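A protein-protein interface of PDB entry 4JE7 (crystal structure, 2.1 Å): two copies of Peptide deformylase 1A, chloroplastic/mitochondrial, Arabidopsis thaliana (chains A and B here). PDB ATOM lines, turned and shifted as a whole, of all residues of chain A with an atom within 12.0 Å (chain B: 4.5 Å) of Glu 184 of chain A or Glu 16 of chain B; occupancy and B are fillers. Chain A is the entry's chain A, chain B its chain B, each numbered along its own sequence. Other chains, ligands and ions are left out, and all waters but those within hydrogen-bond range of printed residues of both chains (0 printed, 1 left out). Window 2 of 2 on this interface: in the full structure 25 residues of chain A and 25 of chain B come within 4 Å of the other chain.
The backbone carbonyl oxygen (O) of Asp 159 of chain B lies within hydrogen-bond range of the guanidinium group (NH2) of Arg 170 of chain A (2.7 Å).
NH2 of Arg 170 of chain A lies within hydrogen-bond range of O of Gly 160 of chain B, at 3.2 Å.
O of Ala 183 of chain A lies close to SG of Cys 186 of chain A, at 3.7 Å.
Among the printed residues, pairs that only touch across the chains: Arg 170 of chain A with His 15 of chain B (3.4 Å), Pro 181 of chain A with Pro 12 of chain B (3.9 Å), Ala 183 of chain A with His 15 of chain B (3.3 Å) and Glu 184 of chain A with Glu 16 of chain B (3.8 Å).
Of the printed residues of chain B, Arg 170 of chain A touches His 15, Asp 159 and Gly 160.
Printed residues of chain B within 4 Å of Pro 181 of chain A: Pro 12.
Glu 184 of chain A touches just one residue of chain B: Glu 16.
Lys 188 of chain A touches none of the printed residues of chain B.
Printed residues of chain A within 4 Å of Pro 12 of chain B: Pro 181.
No residue of chain A comes within 4 Å of Val 13 of chain B.
Glu 16 of chain B touches just one residue of chain A: Glu 184 (3.8 Å).
No residue of chain A comes within 4 Å of Ala 18 of chain B.
Of the printed residues of chain A, Gly 160 of chain B touches Arg 170.
The nearest printed residue of chain B that does not touch Glu 184 of chain A is His 15 of chain B (4.8 Å).
The nearest printed residue of chain B that does not touch Ala 183 of chain A is Glu 16 of chain B (4.2 Å).
Of the 18 printed residues of chain A, 4 touch a printed residue of chain B.
Hydrophobic or aromatic side chains of chain B within 4 Å of the printed part of chain A: Pro 12 and His 15.
Among the printed residues, no Asp or Glu carboxylate lies within 4 Å of a Lys or Arg side-chain nitrogen of the other chain.
No position is printed for both chains.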
ATOM      1  N   LEU A 106      -2.684   1.401  13.696  1.00  0.00           N
ATOM      2  CA  LEU A 106      -3.217   2.693  14.100  1.00  0.00           C
ATOM      3  C   LEU A 106      -4.163   2.512  15.283  1.00  0.00           C
ATOM      4  O   LEU A 106      -5.205   1.835  15.134  1.00  0.00           O
ATOM      5  CB  LEU A 106      -3.980   3.307  12.922  1.00  0.00           C
ATOM      6  CG  LEU A 106      -4.423   4.769  13.133  1.00  0.00           C
ATOM      7  CD1 LEU A 106      -3.173   5.569  13.244  1.00  0.00           C
ATOM      8  CD2 LEU A 106      -5.278   5.357  12.003  1.00  0.00           C
ATOM      9  N   PHE A 108      -5.242   4.579  19.390  1.00  0.00           N
ATOM     10  CA  PHE A 108      -5.143   5.728  20.291  1.00  0.00           C
ATOM     11  C   PHE A 108      -4.099   5.591  21.373  1.00  0.00           C
ATOM     12  O   PHE A 108      -3.956   4.535  21.954  1.00  0.00           O
ATOM     13  CB  PHE A 108      -6.492   6.042  20.941  1.00  0.00           C
ATOM     14  CG  PHE A 108      -7.418   6.771  20.033  1.00  0.00           C
ATOM     15  CD1 PHE A 108      -8.347   6.082  19.257  1.00  0.00           C
ATOM     16  CD2 PHE A 108      -7.348   8.142  19.908  1.00  0.00           C
ATOM     17  CE1 PHE A 108      -9.219   6.740  18.407  1.00  0.00           C
ATOM     18  CE2 PHE A 108      -8.200   8.815  19.010  1.00  0.00           C
ATOM     19  CZ  PHE A 108      -9.151   8.091  18.264  1.00  0.00           C
ATOM     20  N   VAL A 168      -2.403  11.262  13.623  1.00  0.00           N
ATOM     21  CA  VAL A 168      -3.238  11.304  12.434  1.00  0.00           C
ATOM     22  C   VAL A 168      -4.079  12.563  12.522  1.00  0.00           C
ATOM     23  O   VAL A 168      -4.689  12.807  13.623  1.00  0.00           O
ATOM     24  CB  VAL A 168      -4.128  10.081  12.399  1.00  0.00           C
ATOM     25  CG1 VAL A 168      -5.310  10.271  11.430  1.00  0.00           C
ATOM     26  CG2 VAL A 168      -3.336   8.898  11.993  1.00  0.00           C
ATOM     27  N   PRO A 169      -4.096  13.400  11.436  1.00  0.00           N
ATOM     28  CA  PRO A 169      -4.851  14.650  11.527  1.00  0.00           C
ATOM     29  C   PRO A 169      -6.332  14.414  11.799  1.00  0.00           C
ATOM     30  O   PRO A 169      -6.890  13.445  11.285  1.00  0.00           O
ATOM     31  CB  PRO A 169      -4.634  15.322  10.147  1.00  0.00           C
ATOM     32  CG  PRO A 169      -3.436  14.784   9.651  1.00  0.00           C
ATOM     33  CD  PRO A 169      -3.367  13.338  10.152  1.00  0.00           C
ATOM     34  N   ARG A 170      -6.953  15.292  12.604  1.00  0.00           N
ATOM     35  CA  ARG A 170      -8.388  15.250  12.896  1.00  0.00           C
ATOM     36  C   ARG A 170      -8.799  14.205  13.891  1.00  0.00           C
ATOM     37  O   ARG A 170      -9.996  13.874  13.967  1.00  0.00           O
ATOM     38  CB  ARG A 170      -9.252  15.086  11.605  1.00  0.00           C
ATOM     39  CG  ARG A 170      -9.111  16.257  10.624  1.00  0.00           C
ATOM     40  CD  ARG A 170     -10.147  16.305   9.532  1.00  0.00           C
ATOM     41  NE  ARG A 170      -9.460  16.684   8.296  1.00  0.00           N
ATOM     42  CZ  ARG A 170      -9.632  17.823   7.641  1.00  0.00           C
ATOM     43  NH1 ARG A 170      -8.947  18.093   6.529  1.00  0.00           N
ATOM     44  NH2 ARG A 170     -10.507  18.692   8.090  1.00  0.00           N
ATOM     45  N   THR A 171      -7.846  13.654  14.649  1.00  0.00           N
ATOM     46  CA  THR A 171      -8.170  12.594  15.661  1.00  0.00           C
ATOM     47  C   THR A 171      -7.885  13.041  17.118  1.00  0.00           C
ATOM     48  O   THR A 171      -8.266  12.365  18.069  1.00  0.00           O
ATOM     49  CB  THR A 171      -7.478  11.193  15.348  1.00  0.00           C
ATOM     50  OG1 THR A 171      -6.071  11.283  15.565  1.00  0.00           O
ATOM     51  CG2 THR A 171      -7.725  10.724  13.889  1.00  0.00           C
ATOM     52  N   PHE A 172      -7.200  14.164  17.304  1.00  0.00           N
ATOM     53  CA  PHE A 172      -6.880  14.618  18.653  1.00  0.00           C
ATOM     54  C   PHE A 172      -8.204  14.778  19.418  1.00  0.00           C
ATOM     55  O   PHE A 172      -9.167  15.337  18.881  1.00  0.00           O
ATOM     56  CB  PHE A 172      -6.142  15.960  18.544  1.00  0.00           C
ATOM     57  CG  PHE A 172      -5.471  16.427  19.820  1.00  0.00           C
ATOM     58  CD1 PHE A 172      -4.395  15.740  20.353  1.00  0.00           C
ATOM     59  CD2 PHE A 172      -5.887  17.579  20.424  1.00  0.00           C
ATOM     60  CE1 PHE A 172      -3.760  16.202  21.487  1.00  0.00           C
ATOM     61  CE2 PHE A 172      -5.241  18.069  21.554  1.00  0.00           C
ATOM     62  CZ  PHE A 172      -4.170  17.379  22.080  1.00  0.00           C
ATOM     63  N   ARG A 173      -8.287  14.280  20.643  1.00  0.00           N
ATOM     64  CA  ARG A 173      -9.579  14.365  21.344  1.00  0.00           C
ATOM     65  C   ARG A 173      -9.369  14.423  22.841  1.00  0.00           C
ATOM     66  O   ARG A 173      -8.302  14.043  23.292  1.00  0.00           O
ATOM     67  CB  ARG A 173     -10.467  13.171  20.966  1.00  0.00           C
ATOM     68  CG  ARG A 173      -9.763  11.794  21.033  1.00  0.00           C
ATOM     69  CD  ARG A 173     -10.691  10.721  20.437  1.00  0.00           C
ATOM     70  NE  ARG A 173     -11.033  11.081  19.074  1.00  0.00           N
ATOM     71  CZ  ARG A 173     -11.969  10.523  18.336  1.00  0.00           C
ATOM     72  NH1 ARG A 173     -12.721   9.532  18.803  1.00  0.00           N
ATOM     73  NH2 ARG A 173     -12.136  10.985  17.113  1.00  0.00           N
ATOM     74  N   LEU A 180     -15.937   8.593  20.490  1.00  0.00           N
ATOM     75  CA  LEU A 180     -16.818   9.251  19.528  1.00  0.00           C
ATOM     76  C   LEU A 180     -16.303   8.944  18.114  1.00  0.00           C
ATOM     77  O   LEU A 180     -15.091   8.698  17.910  1.00  0.00           O
ATOM     78  CB  LEU A 180     -16.910  10.766  19.798  1.00  0.00           C
ATOM     79  CG  LEU A 180     -17.715  11.306  21.019  1.00  0.00           C
ATOM     80  CD1 LEU A 180     -18.033  12.768  20.804  1.00  0.00           C
ATOM     81  CD2 LEU A 180     -18.997  10.581  21.386  1.00  0.00           C
ATOM     82  N   PRO A 181     -17.205   8.944  17.130  1.00  0.00           N
ATOM     83  CA  PRO A 181     -16.806   8.373  15.877  1.00  0.00           C
ATOM     84  C   PRO A 181     -15.606   9.111  15.264  1.00  0.00           C
ATOM     85  O   PRO A 181     -15.467  10.314  15.474  1.00  0.00           O
ATOM     86  CB  PRO A 181     -18.064   8.545  15.014  1.00  0.00           C
ATOM     87  CG  PRO A 181     -19.189   8.670  16.002  1.00  0.00           C
ATOM     88  CD  PRO A 181     -18.581   9.459  17.100  1.00  0.00           C
ATOM     89  N   LEU A 182     -14.711   8.414  14.563  1.00  0.00           N
ATOM     90  CA  LEU A 182     -13.692   9.126  13.770  1.00  0.00           C
ATOM     91  C   LEU A 182     -14.418   9.886  12.702  1.00  0.00           C
ATOM     92  O   LEU A 182     -15.416   9.377  12.186  1.00  0.00           O
ATOM     93  CB  LEU A 182     -12.763   8.152  13.078  1.00  0.00           C
ATOM     94  CG  LEU A 182     -11.668   7.465  13.892  1.00  0.00           C
ATOM     95  CD1 LEU A 182     -10.870   6.646  12.887  1.00  0.00           C
ATOM     96  CD2 LEU A 182     -10.828   8.504  14.577  1.00  0.00           C
ATOM     97  N   ALA A 183     -13.921  11.087  12.367  1.00  0.00           N
ATOM     98  CA  ALA A 183     -14.477  11.962  11.294  1.00  0.00           C
ATOM     99  C   ALA A 183     -14.329  11.336   9.923  1.00  0.00           C
ATOM    100  O   ALA A 183     -13.543  10.426   9.768  1.00  0.00           O
ATOM    101  CB  ALA A 183     -13.745  13.333  11.295  1.00  0.00           C
ATOM    102  N   GLU A 184     -15.077  11.832   8.941  1.00  0.00           N
ATOM    103  CA  GLU A 184     -14.911  11.447   7.551  1.00  0.00           C
ATOM    104  C   GLU A 184     -13.463  11.682   7.054  1.00  0.00           C
ATOM    105  O   GLU A 184     -12.826  12.693   7.385  1.00  0.00           O
ATOM    106  CB  GLU A 184     -15.953  12.201   6.664  1.00  0.00           C
ATOM    107  N   GLY A 185     -12.942  10.714   6.304  1.00  0.00           N
ATOM    108  CA  GLY A 185     -11.547  10.748   5.783  1.00  0.00           C
ATOM    109  C   GLY A 185     -10.398  10.298   6.689  1.00  0.00           C
ATOM    110  O   GLY A 185      -9.255  10.248   6.272  1.00  0.00           O
ATOM    111  N   CYS A 186     -10.692  10.006   7.941  1.00  0.00           N
ATOM    112  CA  CYS A 186      -9.697   9.534   8.873  1.00  0.00           C
ATOM    113  C   CYS A 186      -9.501   8.043   8.649  1.00  0.00           C
ATOM    114  O   CYS A 186     -10.512   7.317   8.573  1.00  0.00           O
ATOM    115  CB  CYS A 186     -10.223   9.716  10.287  1.00  0.00           C
ATOM    116  SG  CYS A 186     -10.118  11.374  10.856  1.00  0.00           S
ATOM    117  N   PRO A 187      -8.231   7.564   8.591  1.00  0.00           N
ATOM    118  CA  PRO A 187      -8.129   6.117   8.449  1.00  0.00           C
ATOM    119  C   PRO A 187      -8.765   5.374   9.669  1.00  0.00           C
ATOM    120  O   PRO A 187      -8.816   5.913  10.775  1.00  0.00           O
ATOM    121  CB  PRO A 187      -6.610   5.873   8.286  1.00  0.00           C
ATOM    122  CG  PRO A 187      -5.948   7.026   8.911  1.00  0.00           C
ATOM    123  CD  PRO A 187      -6.905   8.211   8.672  1.00  0.00           C
ATOM    124  N   LYS A 188      -9.265   4.163   9.454  1.00  0.00           N
ATOM    125  CA  LYS A 188      -9.811   3.354  10.531  1.00  0.00           C
ATOM    126  C   LYS A 188      -8.692   2.773  11.411  1.00  0.00           C
ATOM    127  O   LYS A 188      -7.568   2.543  10.944  1.00  0.00           O
ATOM    128  CB  LYS A 188     -10.691   2.225   9.922  1.00  0.00           C
ATOM    129  N   LEU A 189      -9.010   2.574  12.681  1.00  0.00           N
ATOM    130  CA  LEU A 189      -8.153   1.884  13.634  1.00  0.00           C
ATOM    131  C   LEU A 189      -8.016   0.407  13.286  1.00  0.00           C
ATOM    132  O   LEU A 189      -8.885  -0.148  12.647  1.00  0.00           O
ATOM    133  CB  LEU A 189      -8.695   2.008  15.044  1.00  0.00           C
ATOM    134  CG  LEU A 189      -9.013   3.349  15.734  1.00  0.00           C
ATOM    135  CD1 LEU A 189      -9.337   2.974  17.198  1.00  0.00           C
ATOM    136  CD2 LEU A 189      -7.865   4.393  15.624  1.00  0.00           C
ATOM    137  N   PRO B  12     -17.149  14.789  16.337  1.00  0.00           N
ATOM    138  CA  PRO B  12     -16.934  14.889  14.875  1.00  0.00           C
ATOM    139  C   PRO B  12     -17.357  16.210  14.151  1.00  0.00           C
ATOM    140  O   PRO B  12     -16.758  16.564  13.135  1.00  0.00           O
ATOM    141  CB  PRO B  12     -17.673  13.673  14.318  1.00  0.00           C
ATOM    142  CG  PRO B  12     -18.411  13.068  15.510  1.00  0.00           C
ATOM    143  CD  PRO B  12     -17.758  13.518  16.737  1.00  0.00           C
ATOM    144  N   VAL B  13     -18.345  16.935  14.668  1.00  0.00           N
ATOM    145  CA  VAL B  13     -18.703  18.264  14.091  1.00  0.00           C
ATOM    146  C   VAL B  13     -17.506  19.231  14.046  1.00  0.00           C
ATOM    147  O   VAL B  13     -17.383  20.045  13.123  1.00  0.00           O
ATOM    148  CB  VAL B  13     -19.956  18.927  14.800  1.00  0.00           C
ATOM    149  CG1 VAL B  13     -19.644  19.322  16.258  1.00  0.00           C
ATOM    150  CG2 VAL B  13     -20.485  20.132  13.984  1.00  0.00           C
ATOM    151  N   LEU B  14     -16.566  19.105  14.969  1.00  0.00           N
ATOM    152  CA  LEU B  14     -15.339  19.907  14.881  1.00  0.00           C
ATOM    153  C   LEU B  14     -14.354  19.484  13.792  1.00  0.00           C
ATOM    154  O   LEU B  14     -13.418  20.231  13.480  1.00  0.00           O
ATOM    155  CB  LEU B  14     -14.606  19.926  16.248  1.00  0.00           C
ATOM    156  CG  LEU B  14     -15.196  20.768  17.388  1.00  0.00           C
ATOM    157  CD1 LEU B  14     -14.442  20.548  18.647  1.00  0.00           C
ATOM    158  CD2 LEU B  14     -15.208  22.241  17.064  1.00  0.00           C
ATOM    159  N   HIS B  15     -14.538  18.287  13.223  1.00  0.00           N
ATOM    160  CA  HIS B  15     -13.488  17.630  12.408  1.00  0.00           C
ATOM    161  C   HIS B  15     -14.000  17.335  11.012  1.00  0.00           C
ATOM    162  O   HIS B  15     -13.450  16.497  10.305  1.00  0.00           O
ATOM    163  CB  HIS B  15     -12.965  16.338  13.113  1.00  0.00           C
ATOM    164  CG  HIS B  15     -12.494  16.583  14.516  1.00  0.00           C
ATOM    165  ND1 HIS B  15     -11.363  17.319  14.801  1.00  0.00           N
ATOM    166  CD2 HIS B  15     -13.045  16.259  15.711  1.00  0.00           C
ATOM    167  CE1 HIS B  15     -11.232  17.426  16.112  1.00  0.00           C
ATOM    168  NE2 HIS B  15     -12.236  16.784  16.687  1.00  0.00           N
ATOM    169  N   GLU B  16     -15.073  18.031  10.652  1.00  0.00           N
ATOM    170  CA  GLU B  16     -15.797  17.843   9.422  1.00  0.00           C
ATOM    171  C   GLU B  16     -16.036  19.213   8.785  1.00  0.00           C
ATOM    172  O   GLU B  16     -16.171  20.237   9.491  1.00  0.00           O
ATOM    173  CB  GLU B  16     -17.136  17.155   9.735  1.00  0.00           C
ATOM    174  CG  GLU B  16     -16.973  15.639  10.010  1.00  0.00           C
ATOM    175  CD  GLU B  16     -18.249  14.883  10.377  1.00  0.00           C
ATOM    176  OE1 GLU B  16     -19.266  15.459  10.889  1.00  0.00           O
ATOM    177  OE2 GLU B  16     -18.208  13.649  10.143  1.00  0.00           O
ATOM    178  N   LYS B  17     -16.094  19.232   7.452  1.00  0.00           N
ATOM    179  CA  LYS B  17     -16.369  20.433   6.708  1.00  0.00           C
ATOM    180  C   LYS B  17     -17.813  20.911   6.920  1.00  0.00           C
ATOM    181  O   LYS B  17     -18.772  20.158   6.821  1.00  0.00           O
ATOM    182  CB  LYS B  17     -16.094  20.194   5.245  1.00  0.00           C
ATOM    183  CG  LYS B  17     -15.862  21.460   4.511  1.00  0.00           C
ATOM    184  CD  LYS B  17     -15.886  21.271   3.044  1.00  0.00           C
ATOM    185  CE  LYS B  17     -15.515  22.600   2.406  1.00  0.00           C
ATOM    186  NZ  LYS B  17     -15.216  22.399   0.976  1.00  0.00           N
ATOM    187  N   ALA B  18     -17.953  22.185   7.247  1.00  0.00           N
ATOM    188  CA  ALA B  18     -19.250  22.789   7.547  1.00  0.00           C
ATOM    189  C   ALA B  18     -19.908  23.182   6.233  1.00  0.00           C
ATOM    190  O   ALA B  18     -19.191  23.415   5.241  1.00  0.00           O
ATOM    191  CB  ALA B  18     -19.009  23.967   8.344  1.00  0.00           C
ATOM    192  N   LEU B 158     -13.883  25.851   9.992  1.00  0.00           N
ATOM    193  CA  LEU B 158     -15.031  25.578   9.122  1.00  0.00           C
ATOM    194  C   LEU B 158     -14.712  24.481   8.162  1.00  0.00           C
ATOM    195  O   LEU B 158     -15.620  23.897   7.575  1.00  0.00           O
ATOM    196  CB  LEU B 158     -15.563  26.821   8.389  1.00  0.00           C
ATOM    197  CG  LEU B 158     -16.044  28.012   9.225  1.00  0.00           C
ATOM    198  CD1 LEU B 158     -16.598  29.048   8.207  1.00  0.00           C
ATOM    199  CD2 LEU B 158     -17.075  27.597  10.236  1.00  0.00           C
ATOM    200  N   ASP B 159     -13.417  24.233   7.994  1.00  0.00           N
ATOM    201  CA  ASP B 159     -12.925  23.118   7.164  1.00  0.00           C
ATOM    202  C   ASP B 159     -12.556  21.912   8.053  1.00  0.00           C
ATOM    203  O   ASP B 159     -11.798  21.030   7.630  1.00  0.00           O
ATOM    204  CB  ASP B 159     -11.724  23.551   6.258  1.00  0.00           C
ATOM    205  CG  ASP B 159     -12.181  24.242   4.951  1.00  0.00           C
ATOM    206  OD1 ASP B 159     -11.419  25.044   4.382  1.00  0.00           O
ATOM    207  OD2 ASP B 159     -13.329  23.993   4.509  1.00  0.00           O
ATOM    208  N   GLY B 160     -13.075  21.895   9.276  1.00  0.00           N
ATOM    209  CA  GLY B 160     -12.741  20.827  10.219  1.00  0.00           C
ATOM    210  C   GLY B 160     -11.308  20.749  10.689  1.00  0.00           C
ATOM    211  O   GLY B 160     -10.854  19.679  11.080  1.00  0.00           O
